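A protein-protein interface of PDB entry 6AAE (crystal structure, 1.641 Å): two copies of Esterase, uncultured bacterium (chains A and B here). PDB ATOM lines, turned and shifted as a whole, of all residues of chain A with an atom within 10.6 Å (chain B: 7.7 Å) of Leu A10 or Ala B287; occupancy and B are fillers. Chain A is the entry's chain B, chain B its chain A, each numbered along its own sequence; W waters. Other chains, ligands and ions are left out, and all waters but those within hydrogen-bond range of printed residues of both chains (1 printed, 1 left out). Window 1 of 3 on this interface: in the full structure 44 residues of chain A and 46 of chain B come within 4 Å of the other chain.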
ATOM      1  N   LEU A   3      20.541  42.794  29.340  1.00  0.00           N
ATOM      2  CA  LEU A   3      20.694  41.431  28.866  1.00  0.00           C
ATOM      3  C   LEU A   3      20.452  40.490  30.046  1.00  0.00           C
ATOM      4  O   LEU A   3      20.996  40.687  31.125  1.00  0.00           O
ATOM      5  CB  LEU A   3      22.087  41.241  28.251  1.00  0.00           C
ATOM      6  CG  LEU A   3      22.495  39.895  27.664  1.00  0.00           C
ATOM      7  CD1 LEU A   3      21.621  39.527  26.472  1.00  0.00           C
ATOM      8  CD2 LEU A   3      23.961  39.950  27.257  1.00  0.00           C
ATOM      9  N   ASN A   4      19.596  39.492  29.856  1.00  0.00           N
ATOM     10  CA  ASN A   4      19.280  38.549  30.924  1.00  0.00           C
ATOM     11  C   ASN A   4      20.560  37.892  31.462  1.00  0.00           C
ATOM     12  O   ASN A   4      21.397  37.426  30.694  1.00  0.00           O
ATOM     13  CB  ASN A   4      18.274  37.507  30.407  1.00  0.00           C
ATOM     14  CG  ASN A   4      17.838  36.518  31.480  1.00  0.00           C
ATOM     15  OD1 ASN A   4      18.601  35.647  31.864  1.00  0.00           O
ATOM     16  ND2 ASN A   4      16.603  36.644  31.948  1.00  0.00           N
ATOM     17  N   PRO A   5      20.741  37.903  32.791  1.00  0.00           N
ATOM     18  CA  PRO A   5      21.977  37.425  33.422  1.00  0.00           C
ATOM     19  C   PRO A   5      22.252  35.955  33.151  1.00  0.00           C
ATOM     20  O   PRO A   5      23.403  35.574  32.979  1.00  0.00           O
ATOM     21  CB  PRO A   5      21.720  37.650  34.917  1.00  0.00           C
ATOM     22  CG  PRO A   5      20.660  38.681  34.964  1.00  0.00           C
ATOM     23  CD  PRO A   5      19.781  38.388  33.792  1.00  0.00           C
ATOM     24  N   HIS A   6      21.201  35.141  33.120  1.00  0.00           N
ATOM     25  CA  HIS A   6      21.358  33.736  32.785  1.00  0.00           C
ATOM     26  C   HIS A   6      21.757  33.595  31.323  1.00  0.00           C
ATOM     27  O   HIS A   6      22.571  32.738  30.968  1.00  0.00           O
ATOM     28  CB  HIS A   6      20.067  32.960  33.083  1.00  0.00           C
ATOM     29  CG  HIS A   6      19.812  32.780  34.549  1.00  0.00           C
ATOM     30  ND1 HIS A   6      18.920  33.558  35.255  1.00  0.00           N
ATOM     31  CD2 HIS A   6      20.358  31.926  35.447  1.00  0.00           C
ATOM     32  CE1 HIS A   6      18.919  33.184  36.523  1.00  0.00           C
ATOM     33  NE2 HIS A   6      19.782  32.194  36.665  1.00  0.00           N
ATOM     34  N   VAL A   7      21.192  34.448  30.474  1.00  0.00           N
ATOM     35  CA  VAL A   7      21.561  34.438  29.064  1.00  0.00           C
ATOM     36  C   VAL A   7      23.029  34.819  28.881  1.00  0.00           C
ATOM     37  O   VAL A   7      23.762  34.199  28.103  1.00  0.00           O
ATOM     38  CB  VAL A   7      20.673  35.391  28.256  1.00  0.00           C
ATOM     39  CG1 VAL A   7      21.253  35.610  26.871  1.00  0.00           C
ATOM     40  CG2 VAL A   7      19.242  34.855  28.188  1.00  0.00           C
ATOM     41  N   GLU A   8      23.456  35.846  29.607  1.00  0.00           N
ATOM     42  CA  GLU A   8      24.837  36.299  29.551  1.00  0.00           C
ATOM     43  C   GLU A   8      25.807  35.182  29.956  1.00  0.00           C
ATOM     44  O   GLU A   8      26.847  35.000  29.324  1.00  0.00           O
ATOM     45  CB  GLU A   8      25.029  37.530  30.443  1.00  0.00           C
ATOM     46  CG  GLU A   8      26.093  38.496  29.951  1.00  0.00           C
ATOM     47  CD  GLU A   8      27.341  38.444  30.791  1.00  0.00           C
ATOM     48  OE1 GLU A   8      27.337  37.696  31.794  1.00  0.00           O
ATOM     49  OE2 GLU A   8      28.320  39.149  30.456  1.00  0.00           O
ATOM     50  N   ALA A   9      25.454  34.416  30.983  1.00  0.00           N
ATOM     51  CA  ALA A   9      26.278  33.280  31.404  1.00  0.00           C
ATOM     52  C   ALA A   9      26.331  32.186  30.340  1.00  0.00           C
ATOM     53  O   ALA A   9      27.370  31.551  30.137  1.00  0.00           O
ATOM     54  CB  ALA A   9      25.763  32.708  32.708  1.00  0.00           C
ATOM     55  N   LEU A  10      25.208  31.954  29.672  1.00  0.00           N
ATOM     56  CA  LEU A  10      25.168  30.982  28.590  1.00  0.00           C
ATOM     57  C   LEU A  10      26.020  31.447  27.409  1.00  0.00           C
ATOM     58  O   LEU A  10      26.710  30.642  26.784  1.00  0.00           O
ATOM     59  CB  LEU A  10      23.723  30.734  28.147  1.00  0.00           C
ATOM     60  CG  LEU A  10      23.517  29.570  27.182  1.00  0.00           C
ATOM     61  CD1 LEU A  10      23.948  28.271  27.850  1.00  0.00           C
ATOM     62  CD2 LEU A  10      22.061  29.489  26.743  1.00  0.00           C
ATOM     63  N   LEU A  11      25.980  32.746  27.114  1.00  0.00           N
ATOM     64  CA  LEU A  11      26.777  33.307  26.022  1.00  0.00           C
ATOM     65  C   LEU A  11      28.281  33.202  26.299  1.00  0.00           C
ATOM     66  O   LEU A  11      29.065  32.927  25.390  1.00  0.00           O
ATOM     67  CB  LEU A  11      26.391  34.767  25.765  1.00  0.00           C
ATOM     68  CG  LEU A  11      25.093  35.010  24.989  1.00  0.00           C
ATOM     69  CD1 LEU A  11      24.710  36.471  25.039  1.00  0.00           C
ATOM     70  CD2 LEU A  11      25.222  34.544  23.544  1.00  0.00           C
ATOM     71  N   GLN A  12      28.676  33.422  27.550  1.00  0.00           N
ATOM     72  CA  GLN A  12      30.078  33.249  27.947  1.00  0.00           C
ATOM     73  C   GLN A  12      30.529  31.808  27.760  1.00  0.00           C
ATOM     74  O   GLN A  12      31.651  31.544  27.337  1.00  0.00           O
ATOM     75  CB  GLN A  12      30.291  33.646  29.403  1.00  0.00           C
ATOM     76  CG  GLN A  12      30.104  35.111  29.708  1.00  0.00           C
ATOM     77  CD  GLN A  12      30.381  35.405  31.166  1.00  0.00           C
ATOM     78  OE1 GLN A  12      31.406  34.984  31.706  1.00  0.00           O
ATOM     79  NE2 GLN A  12      29.469  36.118  31.817  1.00  0.00           N
ATOM     80  N   MET A  13      29.639  30.881  28.109  1.00  0.00           N
ATOM     81  CA  MET A  13      29.870  29.458  27.929  1.00  0.00           C
ATOM     82  C   MET A  13      30.026  29.154  26.445  1.00  0.00           C
ATOM     83  O   MET A  13      30.904  28.389  26.042  1.00  0.00           O
ATOM     84  CB  MET A  13      28.711  28.664  28.545  1.00  0.00           C
ATOM     85  CG  MET A  13      28.899  27.166  28.623  1.00  0.00           C
ATOM     86  SD  MET A  13      27.537  26.380  29.514  1.00  0.00           S
ATOM     87  CE  MET A  13      28.014  26.723  31.211  1.00  0.00           C
ATOM     88  N   MET A  14      29.174  29.781  25.638  1.00  0.00           N
ATOM     89  CA  MET A  14      29.228  29.659  24.182  1.00  0.00           C
ATOM     90  C   MET A  14      30.468  30.324  23.589  1.00  0.00           C
ATOM     91  O   MET A  14      30.904  29.979  22.498  1.00  0.00           O
ATOM     92  CB  MET A  14      27.987  30.284  23.542  1.00  0.00           C
ATOM     93  CG  MET A  14      26.697  29.504  23.687  1.00  0.00           C
ATOM     94  SD  MET A  14      25.370  30.497  22.967  1.00  0.00           S
ATOM     95  CE  MET A  14      23.950  29.427  23.157  1.00  0.00           C
ATOM     96  N   ALA A  15      31.028  31.300  24.292  1.00  0.00           N
ATOM     97  CA  ALA A  15      32.192  32.004  23.768  1.00  0.00           C
ATOM     98  C   ALA A  15      33.474  31.181  23.931  1.00  0.00           C
ATOM     99  O   ALA A  15      34.575  31.692  23.732  1.00  0.00           O
ATOM    100  CB  ALA A  15      32.337  33.356  24.441  1.00  0.00           C
ATOM    101  N   GLN A  16      33.326  29.907  24.287  1.00  0.00           N
ATOM    102  CA  GLN A  16      34.470  29.013  24.452  1.00  0.00           C
ATOM    103  C   GLN A  16      34.295  27.723  23.652  1.00  0.00           C
ATOM    104  O   GLN A  16      34.214  26.640  24.239  1.00  0.00           O
ATOM    105  CB  GLN A  16      34.675  28.678  25.930  1.00  0.00           C
ATOM    106  CG  GLN A  16      34.963  29.880  26.808  1.00  0.00           C
ATOM    107  CD  GLN A  16      36.398  29.908  27.292  1.00  0.00           C
ATOM    108  OE1 GLN A  16      36.857  28.983  27.966  1.00  0.00           O
ATOM    109  NE2 GLN A  16      37.119  30.970  26.947  1.00  0.00           N
ATOM    110  N   MET A  17      34.270  27.846  22.323  1.00  0.00           N
ATOM    111  CA  MET A  17      33.888  26.750  21.432  1.00  0.00           C
ATOM    112  C   MET A  17      33.892  27.246  19.956  1.00  0.00           C
ATOM    113  O   MET A  17      34.251  28.397  19.719  1.00  0.00           O
ATOM    114  CB  MET A  17      32.526  26.209  21.876  1.00  0.00           C
ATOM    115  CG  MET A  17      31.403  27.191  21.741  1.00  0.00           C
ATOM    116  SD  MET A  17      29.831  26.424  22.131  1.00  0.00           S
ATOM    117  CE  MET A  17      29.728  25.340  20.744  1.00  0.00           C
ATOM    118  N   LEU A  37      25.758  20.226  19.366  1.00  0.00           N
ATOM    119  CA  LEU A  37      25.924  21.024  20.566  1.00  0.00           C
ATOM    120  C   LEU A  37      24.553  21.319  21.170  1.00  0.00           C
ATOM    121  O   LEU A  37      23.584  21.552  20.440  1.00  0.00           O
ATOM    122  CB  LEU A  37      26.682  22.298  20.232  1.00  0.00           C
ATOM    123  CG  LEU A  37      28.000  21.952  19.539  1.00  0.00           C
ATOM    124  CD1 LEU A  37      28.389  23.089  18.655  1.00  0.00           C
ATOM    125  CD2 LEU A  37      29.104  21.671  20.541  1.00  0.00           C
ATOM    126  N   ALA A  38      24.475  21.265  22.499  1.00  0.00           N
ATOM    127  CA  ALA A  38      23.218  21.446  23.231  1.00  0.00           C
ATOM    128  C   ALA A  38      22.081  20.536  22.738  1.00  0.00           C
ATOM    129  O   ALA A  38      20.909  20.922  22.773  1.00  0.00           O
ATOM    130  CB  ALA A  38      22.777  22.903  23.162  1.00  0.00           C
ATOM    131  N   GLU A 286      27.207  18.159  27.020  1.00  0.00           N
ATOM    132  CA  GLU A 286      26.749  19.354  26.311  1.00  0.00           C
ATOM    133  C   GLU A 286      27.432  20.606  26.839  1.00  0.00           C
ATOM    134  O   GLU A 286      27.823  21.464  26.064  1.00  0.00           O
ATOM    135  CB  GLU A 286      25.231  19.504  26.414  1.00  0.00           C
ATOM    136  CG  GLU A 286      24.471  18.339  25.825  1.00  0.00           C
ATOM    137  CD  GLU A 286      22.981  18.588  25.776  1.00  0.00           C
ATOM    138  OE1 GLU A 286      22.556  19.725  26.088  1.00  0.00           O
ATOM    139  OE2 GLU A 286      22.240  17.650  25.419  1.00  0.00           O
ATOM    140  N   ALA A 287      27.589  20.709  28.154  1.00  0.00           N
ATOM    141  CA  ALA A 287      28.237  21.883  28.732  1.00  0.00           C
ATOM    142  C   ALA A 287      29.747  21.700  28.850  1.00  0.00           C
ATOM    143  O   ALA A 287      30.498  22.674  28.969  1.00  0.00           O
ATOM    144  CB  ALA A 287      27.643  22.201  30.097  1.00  0.00           C
ATOM    145  N   VAL A 288      30.187  20.448  28.844  1.00  0.00           N
ATOM    146  CA  VAL A 288      31.595  20.102  29.029  1.00  0.00           C
ATOM    147  C   VAL A 288      32.060  19.208  27.878  1.00  0.00           C
ATOM    148  O   VAL A 288      32.089  17.981  28.006  1.00  0.00           O
ATOM    149  CB  VAL A 288      31.807  19.383  30.376  1.00  0.00           C
ATOM    150  CG1 VAL A 288      33.293  19.078  30.624  1.00  0.00           C
ATOM    151  CG2 VAL A 288      31.219  20.218  31.525  1.00  0.00           C
ATOM    152  N   MET B  13      27.005  28.045  36.992  1.00  0.00           N
ATOM    153  CA  MET B  13      25.705  28.240  36.371  1.00  0.00           C
ATOM    154  C   MET B  13      24.617  27.517  37.148  1.00  0.00           C
ATOM    155  O   MET B  13      23.532  28.059  37.349  1.00  0.00           O
ATOM    156  CB  MET B  13      25.714  27.768  34.918  1.00  0.00           C
ATOM    157  CG  MET B  13      24.322  27.658  34.320  1.00  0.00           C
ATOM    158  SD  MET B  13      24.365  27.300  32.557  1.00  0.00           S
ATOM    159  CE  MET B  13      25.109  28.806  31.932  1.00  0.00           C
ATOM    160  N   GLN B  16      23.463  29.553  40.156  1.00  0.00           N
ATOM    161  CA  GLN B  16      22.621  30.729  39.934  1.00  0.00           C
ATOM    162  C   GLN B  16      21.182  30.364  39.577  1.00  0.00           C
ATOM    163  O   GLN B  16      20.379  31.238  39.258  1.00  0.00           O
ATOM    164  CB  GLN B  16      23.207  31.607  38.828  1.00  0.00           C
ATOM    165  CG  GLN B  16      24.544  32.228  39.166  1.00  0.00           C
ATOM    166  CD  GLN B  16      24.454  33.202  40.327  1.00  0.00           C
ATOM    167  OE1 GLN B  16      24.803  32.866  41.460  1.00  0.00           O
ATOM    168  NE2 GLN B  16      23.986  34.418  40.051  1.00  0.00           N
ATOM    169  N   MET B  17      20.857  29.078  39.621  1.00  0.00           N
ATOM    170  CA  MET B  17      19.513  28.631  39.280  1.00  0.00           C
ATOM    171  C   MET B  17      18.593  28.698  40.500  1.00  0.00           C
ATOM    172  O   MET B  17      19.062  28.641  41.638  1.00  0.00           O
ATOM    173  CB  MET B  17      19.553  27.211  38.706  1.00  0.00           C
ATOM    174  CG  MET B  17      20.371  27.097  37.428  1.00  0.00           C
ATOM    175  SD  MET B  17      19.715  28.099  36.078  1.00  0.00           S
ATOM    176  CE  MET B  17      18.246  27.155  35.679  1.00  0.00           C
ATOM    177  N   PRO B  18      17.279  28.850  40.263  1.00  0.00           N
ATOM    178  CA  PRO B  18      16.301  28.881  41.357  1.00  0.00           C
ATOM    179  C   PRO B  18      16.374  27.630  42.237  1.00  0.00           C
ATOM    180  O   PRO B  18      16.299  26.522  41.711  1.00  0.00           O
ATOM    181  CB  PRO B  18      14.959  28.959  40.619  1.00  0.00           C
ATOM    182  CG  PRO B  18      15.287  29.615  39.320  1.00  0.00           C
ATOM    183  CD  PRO B  18      16.649  29.105  38.953  1.00  0.00           C
ATOM    184  N   TYR B 202      24.803  35.254  19.642  1.00  0.00           N
ATOM    185  CA  TYR B 202      24.616  33.932  19.023  1.00  0.00           C
ATOM    186  C   TYR B 202      24.345  34.059  17.513  1.00  0.00           C
ATOM    187  O   TYR B 202      25.230  33.802  16.700  1.00  0.00           O
ATOM    188  CB  TYR B 202      23.489  33.170  19.734  1.00  0.00           C
ATOM    189  CG  TYR B 202      23.269  31.741  19.289  1.00  0.00           C
ATOM    190  CD1 TYR B 202      24.329  30.946  18.870  1.00  0.00           C
ATOM    191  CD2 TYR B 202      21.992  31.190  19.290  1.00  0.00           C
ATOM    192  CE1 TYR B 202      24.126  29.632  18.465  1.00  0.00           C
ATOM    193  CE2 TYR B 202      21.776  29.877  18.888  1.00  0.00           C
ATOM    194  CZ  TYR B 202      22.849  29.105  18.476  1.00  0.00           C
ATOM    195  OH  TYR B 202      22.648  27.802  18.074  1.00  0.00           O
ATOM    196  N   ILE B 278      17.805  36.607  23.881  1.00  0.00           N
ATOM    197  CA  ILE B 278      18.457  36.515  22.584  1.00  0.00           C
ATOM    198  C   ILE B 278      17.695  35.570  21.666  1.00  0.00           C
ATOM    199  O   ILE B 278      16.792  34.869  22.106  1.00  0.00           O
ATOM    200  CB  ILE B 278      19.901  36.021  22.699  1.00  0.00           C
ATOM    201  CG1 ILE B 278      19.943  34.649  23.392  1.00  0.00           C
ATOM    202  CG2 ILE B 278      20.775  37.060  23.428  1.00  0.00           C
ATOM    203  CD1 ILE B 278      21.292  33.977  23.289  1.00  0.00           C
ATOM    204  N   GLY B 280      16.760  32.326  19.875  1.00  0.00           N
ATOM    205  CA  GLY B 280      16.897  30.953  20.307  1.00  0.00           C
ATOM    206  C   GLY B 280      16.485  30.652  21.735  1.00  0.00           C
ATOM    207  O   GLY B 280      16.569  29.500  22.161  1.00  0.00           O
ATOM    208  N   PHE B 281      16.003  31.644  22.478  1.00  0.00           N
ATOM    209  CA  PHE B 281      15.828  31.443  23.918  1.00  0.00           C
ATOM    210  C   PHE B 281      14.712  30.466  24.314  1.00  0.00           C
ATOM    211  O   PHE B 281      14.686  30.009  25.456  1.00  0.00           O
ATOM    212  CB  PHE B 281      15.613  32.792  24.629  1.00  0.00           C
ATOM    213  CG  PHE B 281      14.230  33.363  24.495  1.00  0.00           C
ATOM    214  CD1 PHE B 281      13.873  34.106  23.381  1.00  0.00           C
ATOM    215  CD2 PHE B 281      13.308  33.216  25.520  1.00  0.00           C
ATOM    216  CE1 PHE B 281      12.611  34.658  23.274  1.00  0.00           C
ATOM    217  CE2 PHE B 281      12.058  33.777  25.421  1.00  0.00           C
ATOM    218  CZ  PHE B 281      11.703  34.493  24.295  1.00  0.00           C
ATOM    219  N   SER B 283      14.616  27.558  23.245  1.00  0.00           N
ATOM    220  CA  SER B 283      15.338  26.303  23.393  1.00  0.00           C
ATOM    221  C   SER B 283      16.346  26.327  24.542  1.00  0.00           C
ATOM    222  O   SER B 283      17.035  25.339  24.785  1.00  0.00           O
ATOM    223  CB  SER B 283      16.050  25.960  22.088  1.00  0.00           C
ATOM    224  OG  SER B 283      15.114  25.948  21.022  1.00  0.00           O
ATOM    225  N   MET B 284      16.429  27.446  25.254  1.00  0.00           N
ATOM    226  CA  MET B 284      17.455  27.603  26.285  1.00  0.00           C
ATOM    227  C   MET B 284      16.879  27.555  27.698  1.00  0.00           C
ATOM    228  O   MET B 284      17.524  28.003  28.643  1.00  0.00           O
ATOM    229  CB  MET B 284      18.209  28.928  26.084  1.00  0.00           C
ATOM    230  CG  MET B 284      18.983  29.000  24.786  1.00  0.00           C
ATOM    231  SD  MET B 284      19.396  30.723  24.378  1.00  0.00           S
ATOM    232  CE  MET B 284      20.149  30.485  22.777  1.00  0.00           C
ATOM    233  N   PHE B 285      15.676  27.001  27.847  1.00  0.00           N
ATOM    234  CA  PHE B 285      14.968  27.026  29.129  1.00  0.00           C
ATOM    235  C   PHE B 285      15.699  26.317  30.277  1.00  0.00           C
ATOM    236  O   PHE B 285      15.440  26.605  31.442  1.00  0.00           O
ATOM    237  CB  PHE B 285      13.564  26.415  28.964  1.00  0.00           C
ATOM    238  CG  PHE B 285      13.575  25.025  28.400  1.00  0.00           C
ATOM    239  CD1 PHE B 285      13.754  23.920  29.226  1.00  0.00           C
ATOM    240  CD2 PHE B 285      13.444  24.826  27.038  1.00  0.00           C
ATOM    241  CE1 PHE B 285      13.787  22.637  28.695  1.00  0.00           C
ATOM    242  CE2 PHE B 285      13.462  23.542  26.502  1.00  0.00           C
ATOM    243  CZ  PHE B 285      13.641  22.451  27.329  1.00  0.00           C
ATOM    244  N   GLU B 286      16.596  25.390  29.968  1.00  0.00           N
ATOM    245  CA  GLU B 286      17.351  24.719  31.025  1.00  0.00           C
ATOM    246  C   GLU B 286      18.366  25.657  31.686  1.00  0.00           C
ATOM    247  O   GLU B 286      18.575  25.588  32.889  1.00  0.00           O
ATOM    248  CB  GLU B 286      18.046  23.478  30.470  1.00  0.00           C
ATOM    249  CG  GLU B 286      17.058  22.342  30.212  1.00  0.00           C
ATOM    250  CD  GLU B 286      17.644  21.202  29.403  1.00  0.00           C
ATOM    251  OE1 GLU B 286      18.685  21.408  28.737  1.00  0.00           O
ATOM    252  OE2 GLU B 286      17.059  20.094  29.436  1.00  0.00           O
ATOM    253  N   ALA B 287      18.981  26.536  30.900  1.00  0.00           N
ATOM    254  CA  ALA B 287      19.957  27.493  31.429  1.00  0.00           C
ATOM    255  C   ALA B 287      19.316  28.833  31.754  1.00  0.00           C
ATOM    256  O   ALA B 287      19.887  29.641  32.494  1.00  0.00           O
ATOM    257  CB  ALA B 287      21.085  27.693  30.447  1.00  0.00           C
ATOM    258  N   VAL B 288      18.133  29.069  31.192  1.00  0.00           N
ATOM    259  CA  VAL B 288      17.465  30.361  31.300  1.00  0.00           C
ATOM    260  C   VAL B 288      16.020  30.153  31.739  1.00  0.00           C
ATOM    261  O   VAL B 288      15.115  30.066  30.911  1.00  0.00           O
ATOM    262  CB  VAL B 288      17.505  31.135  29.956  1.00  0.00           C
ATOM    263  CG1 VAL B 288      16.958  32.557  30.121  1.00  0.00           C
ATOM    264  CG2 VAL B 288      18.930  31.154  29.382  1.00  0.00           C
ATOM    265  N   PRO B 289      15.800  30.045  33.055  1.00  0.00           N
ATOM    266  CA  PRO B 289      14.464  29.744  33.593  1.00  0.00           C
ATOM    267  C   PRO B 289      13.404  30.755  33.167  1.00  0.00           C
ATOM    268  O   PRO B 289      12.219  30.412  33.071  1.00  0.00           O
ATOM    269  CB  PRO B 289      14.676  29.773  35.117  1.00  0.00           C
ATOM    270  CG  PRO B 289      16.032  30.357  35.338  1.00  0.00           C
ATOM    271  CD  PRO B 289      16.829  30.067  34.105  1.00  0.00           C
ATOM    272  N   ASP B 290      13.830  31.976  32.869  1.00  0.00           N
ATOM    273  CA  ASP B 290      12.922  33.015  32.428  1.00  0.00           C
ATOM    274  C   ASP B 290      12.242  32.663  31.094  1.00  0.00           C
ATOM    275  O   ASP B 290      11.151  33.150  30.796  1.00  0.00           O
ATOM    276  CB  ASP B 290      13.686  34.341  32.324  1.00  0.00           C
ATOM    277  CG  ASP B 290      14.381  34.722  33.633  1.00  0.00           C
ATOM    278  OD1 ASP B 290      15.537  34.278  33.875  1.00  0.00           O
ATOM    279  OD2 ASP B 290      13.757  35.462  34.425  1.00  0.00           O
ATOM    280  N   SER B 291      12.875  31.796  30.305  1.00  0.00           N
ATOM    281  CA  SER B 291      12.293  31.375  29.030  1.00  0.00           C
ATOM    282  C   SER B 291      10.930  30.730  29.221  1.00  0.00           C
ATOM    283  O   SER B 291      10.066  30.823  28.351  1.00  0.00           O
ATOM    284  CB  SER B 291      13.212  30.389  28.308  1.00  0.00           C
ATOM    285  OG  SER B 291      14.423  31.011  27.932  1.00  0.00           O
ATOM    286  N   TRP B 292      10.748  30.056  30.353  1.00  0.00           N
ATOM    287  CA  TRP B 292       9.492  29.357  30.602  1.00  0.00           C
ATOM    288  C   TRP B 292       8.293  30.295  30.592  1.00  0.00           C
ATOM    289  O   TRP B 292       7.203  29.891  30.186  1.00  0.00           O
ATOM    290  CB  TRP B 292       9.547  28.605  31.929  1.00  0.00           C
ATOM    291  CG  TRP B 292      10.257  27.304  31.839  1.00  0.00           C
ATOM    292  CD1 TRP B 292      11.487  27.000  32.345  1.00  0.00           C
ATOM    293  CD2 TRP B 292       9.789  26.118  31.185  1.00  0.00           C
ATOM    294  NE1 TRP B 292      11.809  25.701  32.055  1.00  0.00           N
ATOM    295  CE2 TRP B 292      10.783  25.135  31.344  1.00  0.00           C
ATOM    296  CE3 TRP B 292       8.624  25.798  30.480  1.00  0.00           C
ATOM    297  CZ2 TRP B 292      10.645  23.840  30.832  1.00  0.00           C
ATOM    298  CZ3 TRP B 292       8.491  24.514  29.968  1.00  0.00           C
ATOM    299  CH2 TRP B 292       9.491  23.553  30.147  1.00  0.00           C
HETATM  300  O   HOH W   1      20.664  22.559  26.783  1.00  0.00           O
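Met A13 touches its own counterpart, Met B13.
Positions printed for both chains: 13, 16, 17, 286, 287 and 288.
Of chain A, only His A6 (3.4 Å) and Leu A10 (3.9 Å) come within 4 Å of Ala B287.
Of chain B, only Met B13 (3.9 Å) comes within 4 Å of Ala A9.
Of chain A, only Leu A10 and Met A14 come within 4 Å of Met B284.
Val B288 touches just these residues of chain A: Asn A4 (3.9 Å) and Val A7 (3.8 Å).
Of the printed residues of chain B, His A6 touches Gln B16 (2.8 Å), Met B17 (3.9 Å), Ala B287 (3.4 Å) and Asp B290 (3.7 Å).
Of the printed residues of chain B, Val A7 touches Ile B278 and Val B288.
Of the printed residues of chain B, Met A14 touches Met B284.
Printed residues of chain A within 4 Å of Asp B290: Asn A4 and His A6.
Of the printed residues of chain A, Met B17 touches His A6.
Pro B289 touches none of the printed residues of chain A.
Gly B280 touches none of the printed residues of chain A.
The nearest printed residue of chain B that does not touch Leu A11 is Met B13 (6.3 Å).
The side-chain amide nitrogen (ND2) of Asn A4 sits at hydrogen-bond distance from the side-chain carboxylate (OD1) of Asp B290, at 3.2 Å.
The backbone carbonyl oxygen of Gln B16 lies within hydrogen-bond range of a ring nitrogen (NE2) of His A6 (2.8 Å).
Hydrophobic or aromatic side chains of chain B within 4 Å of the printed part of chain A: Met B13, Met B17, Ile B278, Met B284, Ala B287 and Val B288.
Hydrophobic or aromatic side chains of chain A that line the printed part of chain B: His A6, Val A7, Leu A10, Leu A11, Met A13 and Met A14.
Among the printed residues, 16 pairs touch across the chains.
Among the printed residues, no Asp or Glu carboxylate lies within 4 Å of a Lys or Arg side-chain nitrogen of the other chain.
Among the printed residues, merely in contact across the chains: His A6 with Ala B287, Met A13 with Met B13, Leu A10 with Met B284, His A6 with Asp B290, Val A7 with Ile B278, Val A7 with Val B288, Leu A10 with Met B13, Leu A10 with Ala B287, Asn A4 with Val B288, Ala A9 with Met B13, His A6 with Met B17, Met A14 with Met B284, Leu A11 with Ile B278 and Leu A11 with Tyr B202.
OD1 of Asn A4 is in hydrogen-bond range of N of Val A7.
The side-chain amide oxygen (OD1) of Asn A4 is in hydrogen-bond range of the backbone NH (N) of His A6 (2.9 Å).
O of Val B288 sits at hydrogen-bond distance from OG of Ser B291 (3.2 Å).
Water W1 lies within hydrogen-bond range of the side-chain carboxylate (OE1) of Glu B286 (3.0 Å) and the side-chain carboxylate (OE1) of Glu A286 (3.5 Å).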
